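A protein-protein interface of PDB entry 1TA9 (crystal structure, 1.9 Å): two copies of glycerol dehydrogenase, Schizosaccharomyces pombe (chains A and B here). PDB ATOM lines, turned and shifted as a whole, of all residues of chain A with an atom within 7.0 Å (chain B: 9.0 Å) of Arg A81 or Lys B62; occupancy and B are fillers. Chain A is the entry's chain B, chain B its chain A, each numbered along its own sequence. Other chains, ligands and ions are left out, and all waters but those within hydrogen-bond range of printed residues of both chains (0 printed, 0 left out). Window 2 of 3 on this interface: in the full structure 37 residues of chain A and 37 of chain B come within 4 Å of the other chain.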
ATOM      1  N   VAL A  73       5.337  28.288   0.252  1.00  0.00           N
ATOM      2  CA  VAL A  73       4.050  27.600   0.193  1.00  0.00           C
ATOM      3  C   VAL A  73       3.649  27.124   1.578  1.00  0.00           C
ATOM      4  O   VAL A  73       4.409  26.419   2.236  1.00  0.00           O
ATOM      5  CB  VAL A  73       4.130  26.386  -0.753  1.00  0.00           C
ATOM      6  CG1 VAL A  73       2.779  25.681  -0.826  1.00  0.00           C
ATOM      7  CG2 VAL A  73       4.578  26.845  -2.134  1.00  0.00           C
ATOM      8  N   GLN A  74       2.447  27.503   1.999  1.00  0.00           N
ATOM      9  CA  GLN A  74       1.932  27.159   3.321  1.00  0.00           C
ATOM     10  C   GLN A  74       0.470  26.690   3.267  1.00  0.00           C
ATOM     11  O   GLN A  74      -0.396  27.387   2.740  1.00  0.00           O
ATOM     12  CB  GLN A  74       2.047  28.395   4.216  1.00  0.00           C
ATOM     13  CG  GLN A  74       1.433  28.272   5.588  1.00  0.00           C
ATOM     14  CD  GLN A  74       1.328  29.617   6.282  1.00  0.00           C
ATOM     15  OE1 GLN A  74       2.283  30.395   6.294  1.00  0.00           O
ATOM     16  NE2 GLN A  74       0.168  29.896   6.869  1.00  0.00           N
ATOM     17  N   GLY A  75       0.193  25.513   3.823  1.00  0.00           N
ATOM     18  CA  GLY A  75      -1.173  25.017   3.816  1.00  0.00           C
ATOM     19  C   GLY A  75      -1.341  23.751   4.634  1.00  0.00           C
ATOM     20  O   GLY A  75      -0.379  23.026   4.872  1.00  0.00           O
ATOM     21  N   ARG A  76      -2.568  23.478   5.066  1.00  0.00           N
ATOM     22  CA  ARG A  76      -2.821  22.291   5.867  1.00  0.00           C
ATOM     23  C   ARG A  76      -2.814  21.050   4.982  1.00  0.00           C
ATOM     24  O   ARG A  76      -3.521  20.994   3.976  1.00  0.00           O
ATOM     25  CB  ARG A  76      -4.162  22.408   6.590  1.00  0.00           C
ATOM     26  CG  ARG A  76      -4.314  21.377   7.690  1.00  0.00           C
ATOM     27  CD  ARG A  76      -5.595  21.546   8.472  1.00  0.00           C
ATOM     28  NE  ARG A  76      -5.505  20.809   9.726  1.00  0.00           N
ATOM     29  CZ  ARG A  76      -6.418  20.835  10.690  1.00  0.00           C
ATOM     30  NH1 ARG A  76      -7.520  21.562  10.556  1.00  0.00           N
ATOM     31  NH2 ARG A  76      -6.214  20.142  11.803  1.00  0.00           N
ATOM     32  N   HIS A  77      -2.007  20.064   5.365  1.00  0.00           N
ATOM     33  CA  HIS A  77      -1.872  18.813   4.618  1.00  0.00           C
ATOM     34  C   HIS A  77      -1.093  19.044   3.327  1.00  0.00           C
ATOM     35  O   HIS A  77      -1.084  18.198   2.435  1.00  0.00           O
ATOM     36  CB  HIS A  77      -3.251  18.228   4.289  1.00  0.00           C
ATOM     37  CG  HIS A  77      -4.117  18.013   5.492  1.00  0.00           C
ATOM     38  ND1 HIS A  77      -3.744  17.198   6.537  1.00  0.00           N
ATOM     39  CD2 HIS A  77      -5.330  18.517   5.820  1.00  0.00           C
ATOM     40  CE1 HIS A  77      -4.692  17.209   7.460  1.00  0.00           C
ATOM     41  NE2 HIS A  77      -5.664  18.002   7.049  1.00  0.00           N
ATOM     42  N   ALA A  78      -0.426  20.192   3.243  1.00  0.00           N
ATOM     43  CA  ALA A  78       0.344  20.550   2.057  1.00  0.00           C
ATOM     44  C   ALA A  78       1.350  19.489   1.625  1.00  0.00           C
ATOM     45  O   ALA A  78       1.584  19.313   0.432  1.00  0.00           O
ATOM     46  CB  ALA A  78       1.058  21.880   2.282  1.00  0.00           C
ATOM     47  N   PHE A  79       1.949  18.783   2.581  1.00  0.00           N
ATOM     48  CA  PHE A  79       2.924  17.757   2.227  1.00  0.00           C
ATOM     49  C   PHE A  79       2.324  16.676   1.329  1.00  0.00           C
ATOM     50  O   PHE A  79       3.059  15.961   0.653  1.00  0.00           O
ATOM     51  CB  PHE A  79       3.530  17.102   3.477  1.00  0.00           C
ATOM     52  CG  PHE A  79       4.469  17.996   4.248  1.00  0.00           C
ATOM     53  CD1 PHE A  79       5.058  19.108   3.649  1.00  0.00           C
ATOM     54  CD2 PHE A  79       4.794  17.702   5.569  1.00  0.00           C
ATOM     55  CE1 PHE A  79       5.959  19.913   4.357  1.00  0.00           C
ATOM     56  CE2 PHE A  79       5.691  18.497   6.282  1.00  0.00           C
ATOM     57  CZ  PHE A  79       6.277  19.607   5.672  1.00  0.00           C
ATOM     58  N   THR A  80       0.997  16.555   1.318  1.00  0.00           N
ATOM     59  CA  THR A  80       0.346  15.554   0.472  1.00  0.00           C
ATOM     60  C   THR A  80       0.254  16.064  -0.961  1.00  0.00           C
ATOM     61  O   THR A  80      -0.200  15.351  -1.855  1.00  0.00           O
ATOM     62  CB  THR A  80      -1.081  15.210   0.959  1.00  0.00           C
ATOM     63  OG1 THR A  80      -1.919  16.368   0.858  1.00  0.00           O
ATOM     64  CG2 THR A  80      -1.051  14.717   2.399  1.00  0.00           C
ATOM     65  N   ARG A  81       0.683  17.305  -1.163  1.00  0.00           N
ATOM     66  CA  ARG A  81       0.682  17.941  -2.479  1.00  0.00           C
ATOM     67  C   ARG A  81       2.116  18.334  -2.840  1.00  0.00           C
ATOM     68  O   ARG A  81       2.334  19.258  -3.619  1.00  0.00           O
ATOM     69  CB  ARG A  81      -0.191  19.204  -2.465  1.00  0.00           C
ATOM     70  CG  ARG A  81      -1.673  18.968  -2.221  1.00  0.00           C
ATOM     71  CD  ARG A  81      -2.455  20.279  -2.272  1.00  0.00           C
ATOM     72  NE  ARG A  81      -2.289  21.084  -1.064  1.00  0.00           N
ATOM     73  CZ  ARG A  81      -2.879  20.815   0.097  1.00  0.00           C
ATOM     74  NH1 ARG A  81      -3.675  19.758   0.210  1.00  0.00           N
ATOM     75  NH2 ARG A  81      -2.683  21.605   1.144  1.00  0.00           N
ATOM     76  N   SER A  82       3.088  17.627  -2.276  1.00  0.00           N
ATOM     77  CA  SER A  82       4.499  17.923  -2.517  1.00  0.00           C
ATOM     78  C   SER A  82       4.942  18.000  -3.978  1.00  0.00           C
ATOM     79  O   SER A  82       5.561  18.981  -4.386  1.00  0.00           O
ATOM     80  CB  SER A  82       5.379  16.908  -1.786  1.00  0.00           C
ATOM     81  OG  SER A  82       5.194  16.988  -0.385  1.00  0.00           O
ATOM     82  N   TYR A  83       4.634  16.975  -4.764  1.00  0.00           N
ATOM     83  CA  TYR A  83       5.054  16.955  -6.164  1.00  0.00           C
ATOM     84  C   TYR A  83       4.660  18.207  -6.938  1.00  0.00           C
ATOM     85  O   TYR A  83       5.442  18.734  -7.725  1.00  0.00           O
ATOM     86  CB  TYR A  83       4.497  15.721  -6.877  1.00  0.00           C
ATOM     87  CG  TYR A  83       5.031  15.578  -8.282  1.00  0.00           C
ATOM     88  CD1 TYR A  83       4.273  15.973  -9.383  1.00  0.00           C
ATOM     89  CD2 TYR A  83       6.317  15.089  -8.509  1.00  0.00           C
ATOM     90  CE1 TYR A  83       4.782  15.889 -10.677  1.00  0.00           C
ATOM     91  CE2 TYR A  83       6.837  14.999  -9.797  1.00  0.00           C
ATOM     92  CZ  TYR A  83       6.064  15.402 -10.875  1.00  0.00           C
ATOM     93  OH  TYR A  83       6.580  15.326 -12.150  1.00  0.00           O
ATOM     94  N   MET A  84       3.439  18.665  -6.707  1.00  0.00           N
ATOM     95  CA  MET A  84       2.889  19.849  -7.353  1.00  0.00           C
ATOM     96  C   MET A  84       3.841  21.045  -7.313  1.00  0.00           C
ATOM     97  O   MET A  84       3.900  21.848  -8.249  1.00  0.00           O
ATOM     98  CB  MET A  84       1.574  20.193  -6.657  1.00  0.00           C
ATOM     99  CG  MET A  84       0.989  21.538  -6.966  1.00  0.00           C
ATOM    100  SD  MET A  84      -0.545  21.702  -6.037  1.00  0.00           S
ATOM    101  CE  MET A  84      -1.239  23.163  -6.811  1.00  0.00           C
ATOM    102  N   TYR A  85       4.590  21.154  -6.225  1.00  0.00           N
ATOM    103  CA  TYR A  85       5.529  22.253  -6.064  1.00  0.00           C
ATOM    104  C   TYR A  85       6.958  21.812  -6.362  1.00  0.00           C
ATOM    105  O   TYR A  85       7.702  22.508  -7.054  1.00  0.00           O
ATOM    106  CB  TYR A  85       5.426  22.796  -4.640  1.00  0.00           C
ATOM    107  CG  TYR A  85       4.019  23.222  -4.273  1.00  0.00           C
ATOM    108  CD1 TYR A  85       3.453  24.370  -4.827  1.00  0.00           C
ATOM    109  CD2 TYR A  85       3.245  22.463  -3.394  1.00  0.00           C
ATOM    110  CE1 TYR A  85       2.150  24.754  -4.513  1.00  0.00           C
ATOM    111  CE2 TYR A  85       1.938  22.839  -3.075  1.00  0.00           C
ATOM    112  CZ  TYR A  85       1.400  23.985  -3.638  1.00  0.00           C
ATOM    113  OH  TYR A  85       0.119  24.370  -3.325  1.00  0.00           O
ATOM    114  N   VAL A  86       7.336  20.646  -5.848  1.00  0.00           N
ATOM    115  CA  VAL A  86       8.682  20.134  -6.060  1.00  0.00           C
ATOM    116  C   VAL A  86       9.019  19.983  -7.541  1.00  0.00           C
ATOM    117  O   VAL A  86      10.172  20.163  -7.940  1.00  0.00           O
ATOM    118  CB  VAL A  86       8.873  18.764  -5.367  1.00  0.00           C
ATOM    119  CG1 VAL A  86      10.239  18.180  -5.723  1.00  0.00           C
ATOM    120  CG2 VAL A  86       8.748  18.922  -3.865  1.00  0.00           C
ATOM    121  N   LYS A 109       5.210  11.532   4.204  1.00  0.00           N
ATOM    122  CA  LYS A 109       4.121  12.090   3.416  1.00  0.00           C
ATOM    123  C   LYS A 109       4.712  12.745   2.169  1.00  0.00           C
ATOM    124  O   LYS A 109       4.161  12.640   1.074  1.00  0.00           O
ATOM    125  CB  LYS A 109       3.347  13.123   4.240  1.00  0.00           C
ATOM    126  CG  LYS A 109       2.740  12.557   5.518  1.00  0.00           C
ATOM    127  CD  LYS A 109       2.013  13.634   6.313  1.00  0.00           C
ATOM    128  CE  LYS A 109       1.522  13.105   7.651  1.00  0.00           C
ATOM    129  NZ  LYS A 109       0.545  11.993   7.497  1.00  0.00           N
ATOM    130  N   SER A 113       4.297  11.361  -1.864  1.00  0.00           N
ATOM    131  CA  SER A 113       3.807  12.234  -2.926  1.00  0.00           C
ATOM    132  C   SER A 113       4.716  12.214  -4.149  1.00  0.00           C
ATOM    133  O   SER A 113       4.249  12.077  -5.279  1.00  0.00           O
ATOM    134  CB  SER A 113       3.681  13.673  -2.412  1.00  0.00           C
ATOM    135  OG  SER A 113       3.293  14.550  -3.454  1.00  0.00           O
ATOM    136  N   LEU A 114       6.017  12.353  -3.920  1.00  0.00           N
ATOM    137  CA  LEU A 114       6.984  12.362  -5.008  1.00  0.00           C
ATOM    138  C   LEU A 114       7.067  10.999  -5.692  1.00  0.00           C
ATOM    139  O   LEU A 114       7.208  10.920  -6.915  1.00  0.00           O
ATOM    140  CB  LEU A 114       8.359  12.781  -4.476  1.00  0.00           C
ATOM    141  CG  LEU A 114       8.376  14.136  -3.753  1.00  0.00           C
ATOM    142  CD1 LEU A 114       9.792  14.464  -3.296  1.00  0.00           C
ATOM    143  CD2 LEU A 114       7.849  15.225  -4.683  1.00  0.00           C
ATOM    144  N   PHE A 212       8.527  25.265   2.253  1.00  0.00           N
ATOM    145  CA  PHE A 212       7.292  24.489   2.159  1.00  0.00           C
ATOM    146  C   PHE A 212       6.825  24.117   3.561  1.00  0.00           C
ATOM    147  O   PHE A 212       7.512  23.389   4.277  1.00  0.00           O
ATOM    148  CB  PHE A 212       7.614  23.245   1.316  1.00  0.00           C
ATOM    149  CG  PHE A 212       6.420  22.431   0.903  1.00  0.00           C
ATOM    150  CD1 PHE A 212       5.204  23.029   0.610  1.00  0.00           C
ATOM    151  CD2 PHE A 212       6.544  21.053   0.746  1.00  0.00           C
ATOM    152  CE1 PHE A 212       4.121  22.262   0.164  1.00  0.00           C
ATOM    153  CE2 PHE A 212       5.474  20.283   0.304  1.00  0.00           C
ATOM    154  CZ  PHE A 212       4.260  20.889   0.012  1.00  0.00           C
ATOM    155  N   ASP A 214       3.661  22.606   6.054  1.00  0.00           N
ATOM    156  CA  ASP A 214       2.391  21.907   6.206  1.00  0.00           C
ATOM    157  C   ASP A 214       1.878  22.323   7.584  1.00  0.00           C
ATOM    158  O   ASP A 214       2.431  21.933   8.610  1.00  0.00           O
ATOM    159  CB  ASP A 214       2.602  20.390   6.132  1.00  0.00           C
ATOM    160  CG  ASP A 214       1.295  19.608   6.204  1.00  0.00           C
ATOM    161  OD1 ASP A 214       1.203  18.540   5.556  1.00  0.00           O
ATOM    162  OD2 ASP A 214       0.365  20.047   6.915  1.00  0.00           O
ATOM    163  N   GLU B  59      -1.621  27.054 -12.510  1.00  0.00           N
ATOM    164  CA  GLU B  59      -1.983  25.967 -11.609  1.00  0.00           C
ATOM    165  C   GLU B  59      -2.555  26.553 -10.319  1.00  0.00           C
ATOM    166  O   GLU B  59      -1.872  27.290  -9.609  1.00  0.00           O
ATOM    167  CB  GLU B  59      -0.758  25.115 -11.305  1.00  0.00           C
ATOM    168  N   GLU B  60      -3.809  26.222 -10.023  1.00  0.00           N
ATOM    169  CA  GLU B  60      -4.475  26.727  -8.826  1.00  0.00           C
ATOM    170  C   GLU B  60      -4.257  25.820  -7.618  1.00  0.00           C
ATOM    171  O   GLU B  60      -4.167  24.598  -7.750  1.00  0.00           O
ATOM    172  CB  GLU B  60      -5.977  26.887  -9.087  1.00  0.00           C
ATOM    173  CG  GLU B  60      -6.731  27.583  -7.965  1.00  0.00           C
ATOM    174  CD  GLU B  60      -8.205  27.769  -8.274  1.00  0.00           C
ATOM    175  OE1 GLU B  60      -8.904  28.425  -7.474  1.00  0.00           O
ATOM    176  OE2 GLU B  60      -8.667  27.254  -9.316  1.00  0.00           O
ATOM    177  N   SER B  61      -4.184  26.430  -6.438  1.00  0.00           N
ATOM    178  CA  SER B  61      -3.969  25.694  -5.197  1.00  0.00           C
ATOM    179  C   SER B  61      -4.735  26.324  -4.038  1.00  0.00           C
ATOM    180  O   SER B  61      -5.173  27.473  -4.118  1.00  0.00           O
ATOM    181  CB  SER B  61      -2.473  25.661  -4.866  1.00  0.00           C
ATOM    182  OG  SER B  61      -2.233  24.982  -3.648  1.00  0.00           O
ATOM    183  N   LYS B  62      -4.889  25.562  -2.960  1.00  0.00           N
ATOM    184  CA  LYS B  62      -5.603  26.023  -1.771  1.00  0.00           C
ATOM    185  C   LYS B  62      -4.611  26.491  -0.705  1.00  0.00           C
ATOM    186  O   LYS B  62      -4.994  26.962   0.366  1.00  0.00           O
ATOM    187  CB  LYS B  62      -6.477  24.889  -1.230  1.00  0.00           C
ATOM    188  CG  LYS B  62      -7.141  25.174   0.104  1.00  0.00           C
ATOM    189  CD  LYS B  62      -6.657  24.206   1.178  1.00  0.00           C
ATOM    190  CE  LYS B  62      -7.081  22.764   0.888  1.00  0.00           C
ATOM    191  NZ  LYS B  62      -6.387  22.176  -0.293  1.00  0.00           N
ATOM    192  N   ASP B  63      -3.329  26.358  -1.009  1.00  0.00           N
ATOM    193  CA  ASP B  63      -2.288  26.776  -0.089  1.00  0.00           C
ATOM    194  C   ASP B  63      -2.033  28.277  -0.235  1.00  0.00           C
ATOM    195  O   ASP B  63      -2.419  28.884  -1.234  1.00  0.00           O
ATOM    196  CB  ASP B  63      -1.007  25.987  -0.375  1.00  0.00           C
ATOM    197  CG  ASP B  63      -1.212  24.483  -0.252  1.00  0.00           C
ATOM    198  OD1 ASP B  63      -1.706  24.035   0.804  1.00  0.00           O
ATOM    199  OD2 ASP B  63      -0.884  23.751  -1.208  1.00  0.00           O
ATOM    200  N   ARG B  64      -1.402  28.869   0.777  1.00  0.00           N
ATOM    201  CA  ARG B  64      -1.069  30.289   0.769  1.00  0.00           C
ATOM    202  C   ARG B  64       0.301  30.367   0.098  1.00  0.00           C
ATOM    203  O   ARG B  64       1.274  29.800   0.595  1.00  0.00           O
ATOM    204  CB  ARG B  64      -0.997  30.815   2.205  1.00  0.00           C
ATOM    205  CG  ARG B  64      -0.808  32.313   2.305  1.00  0.00           C
ATOM    206  CD  ARG B  64      -0.720  32.770   3.762  1.00  0.00           C
ATOM    207  NE  ARG B  64      -1.905  32.408   4.541  1.00  0.00           N
ATOM    208  CZ  ARG B  64      -2.330  33.088   5.603  1.00  0.00           C
ATOM    209  NH1 ARG B  64      -3.411  32.696   6.261  1.00  0.00           N
ATOM    210  NH2 ARG B  64      -1.681  34.179   5.997  1.00  0.00           N
ATOM    211  N   ILE B  65       0.382  31.076  -1.019  1.00  0.00           N
ATOM    212  CA  ILE B  65       1.633  31.137  -1.774  1.00  0.00           C
ATOM    213  C   ILE B  65       2.197  32.530  -2.053  1.00  0.00           C
ATOM    214  O   ILE B  65       1.462  33.445  -2.429  1.00  0.00           O
ATOM    215  CB  ILE B  65       1.443  30.417  -3.141  1.00  0.00           C
ATOM    216  CG1 ILE B  65       0.905  29.003  -2.909  1.00  0.00           C
ATOM    217  CG2 ILE B  65       2.759  30.380  -3.913  1.00  0.00           C
ATOM    218  CD1 ILE B  65       0.502  28.267  -4.191  1.00  0.00           C
ATOM    219  N   THR B 249      -8.451  33.435  -5.970  1.00  0.00           N
ATOM    220  CA  THR B 249      -7.100  32.909  -6.082  1.00  0.00           C
ATOM    221  C   THR B 249      -6.160  33.999  -6.597  1.00  0.00           C
ATOM    222  O   THR B 249      -6.514  34.770  -7.493  1.00  0.00           O
ATOM    223  CB  THR B 249      -7.071  31.710  -7.035  1.00  0.00           C
ATOM    224  OG1 THR B 249      -7.958  30.702  -6.539  1.00  0.00           O
ATOM    225  CG2 THR B 249      -5.663  31.136  -7.138  1.00  0.00           C
ATOM    226  N   ALA B 252      -0.412  34.099  -7.892  1.00  0.00           N
ATOM    227  CA  ALA B 252       0.676  33.234  -7.461  1.00  0.00           C
ATOM    228  C   ALA B 252       0.164  31.791  -7.412  1.00  0.00           C
ATOM    229  O   ALA B 252       0.934  30.859  -7.194  1.00  0.00           O
ATOM    230  CB  ALA B 252       1.189  33.666  -6.089  1.00  0.00           C
ATOM    231  N   GLY B 253      -1.142  31.619  -7.605  1.00  0.00           N
ATOM    232  CA  GLY B 253      -1.715  30.282  -7.613  1.00  0.00           C
ATOM    233  C   GLY B 253      -2.421  29.786  -6.363  1.00  0.00           C
ATOM    234  O   GLY B 253      -2.838  28.627  -6.310  1.00  0.00           O
ATOM    235  N   GLY B 254      -2.571  30.634  -5.354  1.00  0.00           N
ATOM    236  CA  GLY B 254      -3.242  30.180  -4.147  1.00  0.00           C
ATOM    237  C   GLY B 254      -3.919  31.308  -3.398  1.00  0.00           C
ATOM    238  O   GLY B 254      -4.281  32.327  -3.990  1.00  0.00           O
ATOM    239  N   VAL B 255      -4.106  31.116  -2.096  1.00  0.00           N
ATOM    240  CA  VAL B 255      -4.723  32.136  -1.261  1.00  0.00           C
ATOM    241  C   VAL B 255      -3.704  33.250  -1.110  1.00  0.00           C
ATOM    242  O   VAL B 255      -2.510  32.988  -0.940  1.00  0.00           O
ATOM    243  CB  VAL B 255      -5.070  31.584   0.134  1.00  0.00           C
ATOM    244  CG1 VAL B 255      -5.714  32.673   0.980  1.00  0.00           C
ATOM    245  CG2 VAL B 255      -6.003  30.396  -0.002  1.00  0.00           C
ATOM    246  N   ALA B 256      -4.169  34.492  -1.177  1.00  0.00           N
ATOM    247  CA  ALA B 256      -3.275  35.637  -1.061  1.00  0.00           C
ATOM    248  C   ALA B 256      -2.593  35.733   0.298  1.00  0.00           C
ATOM    249  O   ALA B 256      -3.232  35.600   1.341  1.00  0.00           O
ATOM    250  CB  ALA B 256      -4.044  36.926  -1.347  1.00  0.00           C
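OG of Ser B61 lies within hydrogen-bond range of OH of Tyr A85. OD1 of Asp B63 lies within salt-bridge range of NH2 of Arg A81 (2.6 Å). OD2 of Asp B63 lies within hydrogen-bond range of OH of Tyr A85 (2.4 Å). The backbone carbonyl oxygen of Gln A74 sits at hydrogen-bond distance from the backbone NH of Arg B64.
The side-chain hydroxyl (OG1) of Thr B249 lies within hydrogen-bond range of the side-chain carboxylate (OE1) of Glu B60, 2.6 Å away. The side-chain hydroxyl of Ser B61 sits at hydrogen-bond distance from the side-chain carboxylate of Asp B63, at 3.0 Å. N of Ser B61 lies within hydrogen-bond range of O of Gly B253 (2.6 Å). The backbone NH of Val B255 lies within hydrogen-bond range of the backbone carbonyl oxygen of Asp B63. The guanidinium group (NH2) of Arg A81 is in hydrogen-bond range of the backbone carbonyl oxygen (O) of Arg A76 (3.0 Å). N of Ala A78 sits at hydrogen-bond distance from OD1 of Asp A214, at 3.3 Å.
Val A73 touches Asp B63 (CG1 to CB, 3.8 Å). CA of Val A73 touches O of Arg B64, at 3.6 Å. Gln A74 touches Asp B63 (O to CA, 3.5 Å). Asp B63 touches Gly A75. Ala A78 touches Asp B63. Arg A81 touches Lys B62 (NH1 to NZ, 3.7 Å). Met A84 touches Glu B60. Ser B61 touches Met A84 (CB to CE, 3.4 Å). CD1 of Ile B65 touches CE1 of Tyr A85 (3.9 Å).
Arg A81 touches just these residues of chain B: Lys B62 (3.7 Å) and Asp B63 (2.6 Å). Lys B62 touches just one residue of chain A: Arg A81. No residue of chain B comes within 4 Å of Ser A82. Of the printed residues of chain B, Met A84 touches Glu B60 (3.4 Å) and Ser B61 (3.4 Å). Of the printed residues of chain B, Tyr A85 touches Ser B61 (2.5 Å), Asp B63 (2.4 Å) and Ile B65 (3.9 Å). Printed residues of chain B within 4 Å of Gln A74: Asp B63 and Arg B64. Printed residues of chain A within 4 Å of Ile B65: Tyr A85 (3.9 Å). Of the printed residues of chain A, Arg B64 touches Val A73 and Gln A74. Gly B254 touches none of the printed residues of chain A. Leu A114 touches none of the printed residues of chain B. The nearest printed residue of chain B that does not touch Gln A74 is Ile B65 (5.1 Å).
Printed residues of chain B that touch a printed residue of chain A: Glu B60, Ser B61, Lys B62, Asp B63, Arg B64 and Ile B65. Along chain B the printed residues that touch a printed residue of chain A span positions 60 to 65. Hydrophobic or aromatic side chains of chain A within 4 Å of the printed part of chain B: Val A73, Ala A78, Met A84 and Tyr A85. Along chain A the printed residues that touch a printed residue of chain B span positions 73 to 85. Among the printed residues, 13 pairs touch across the chains. Among the printed residues, Asp or Glu carboxylates within 4 Å of a Lys or Arg side-chain nitrogen of the other chain: Arg A81 with Asp B63.
No position is printed for both chains.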
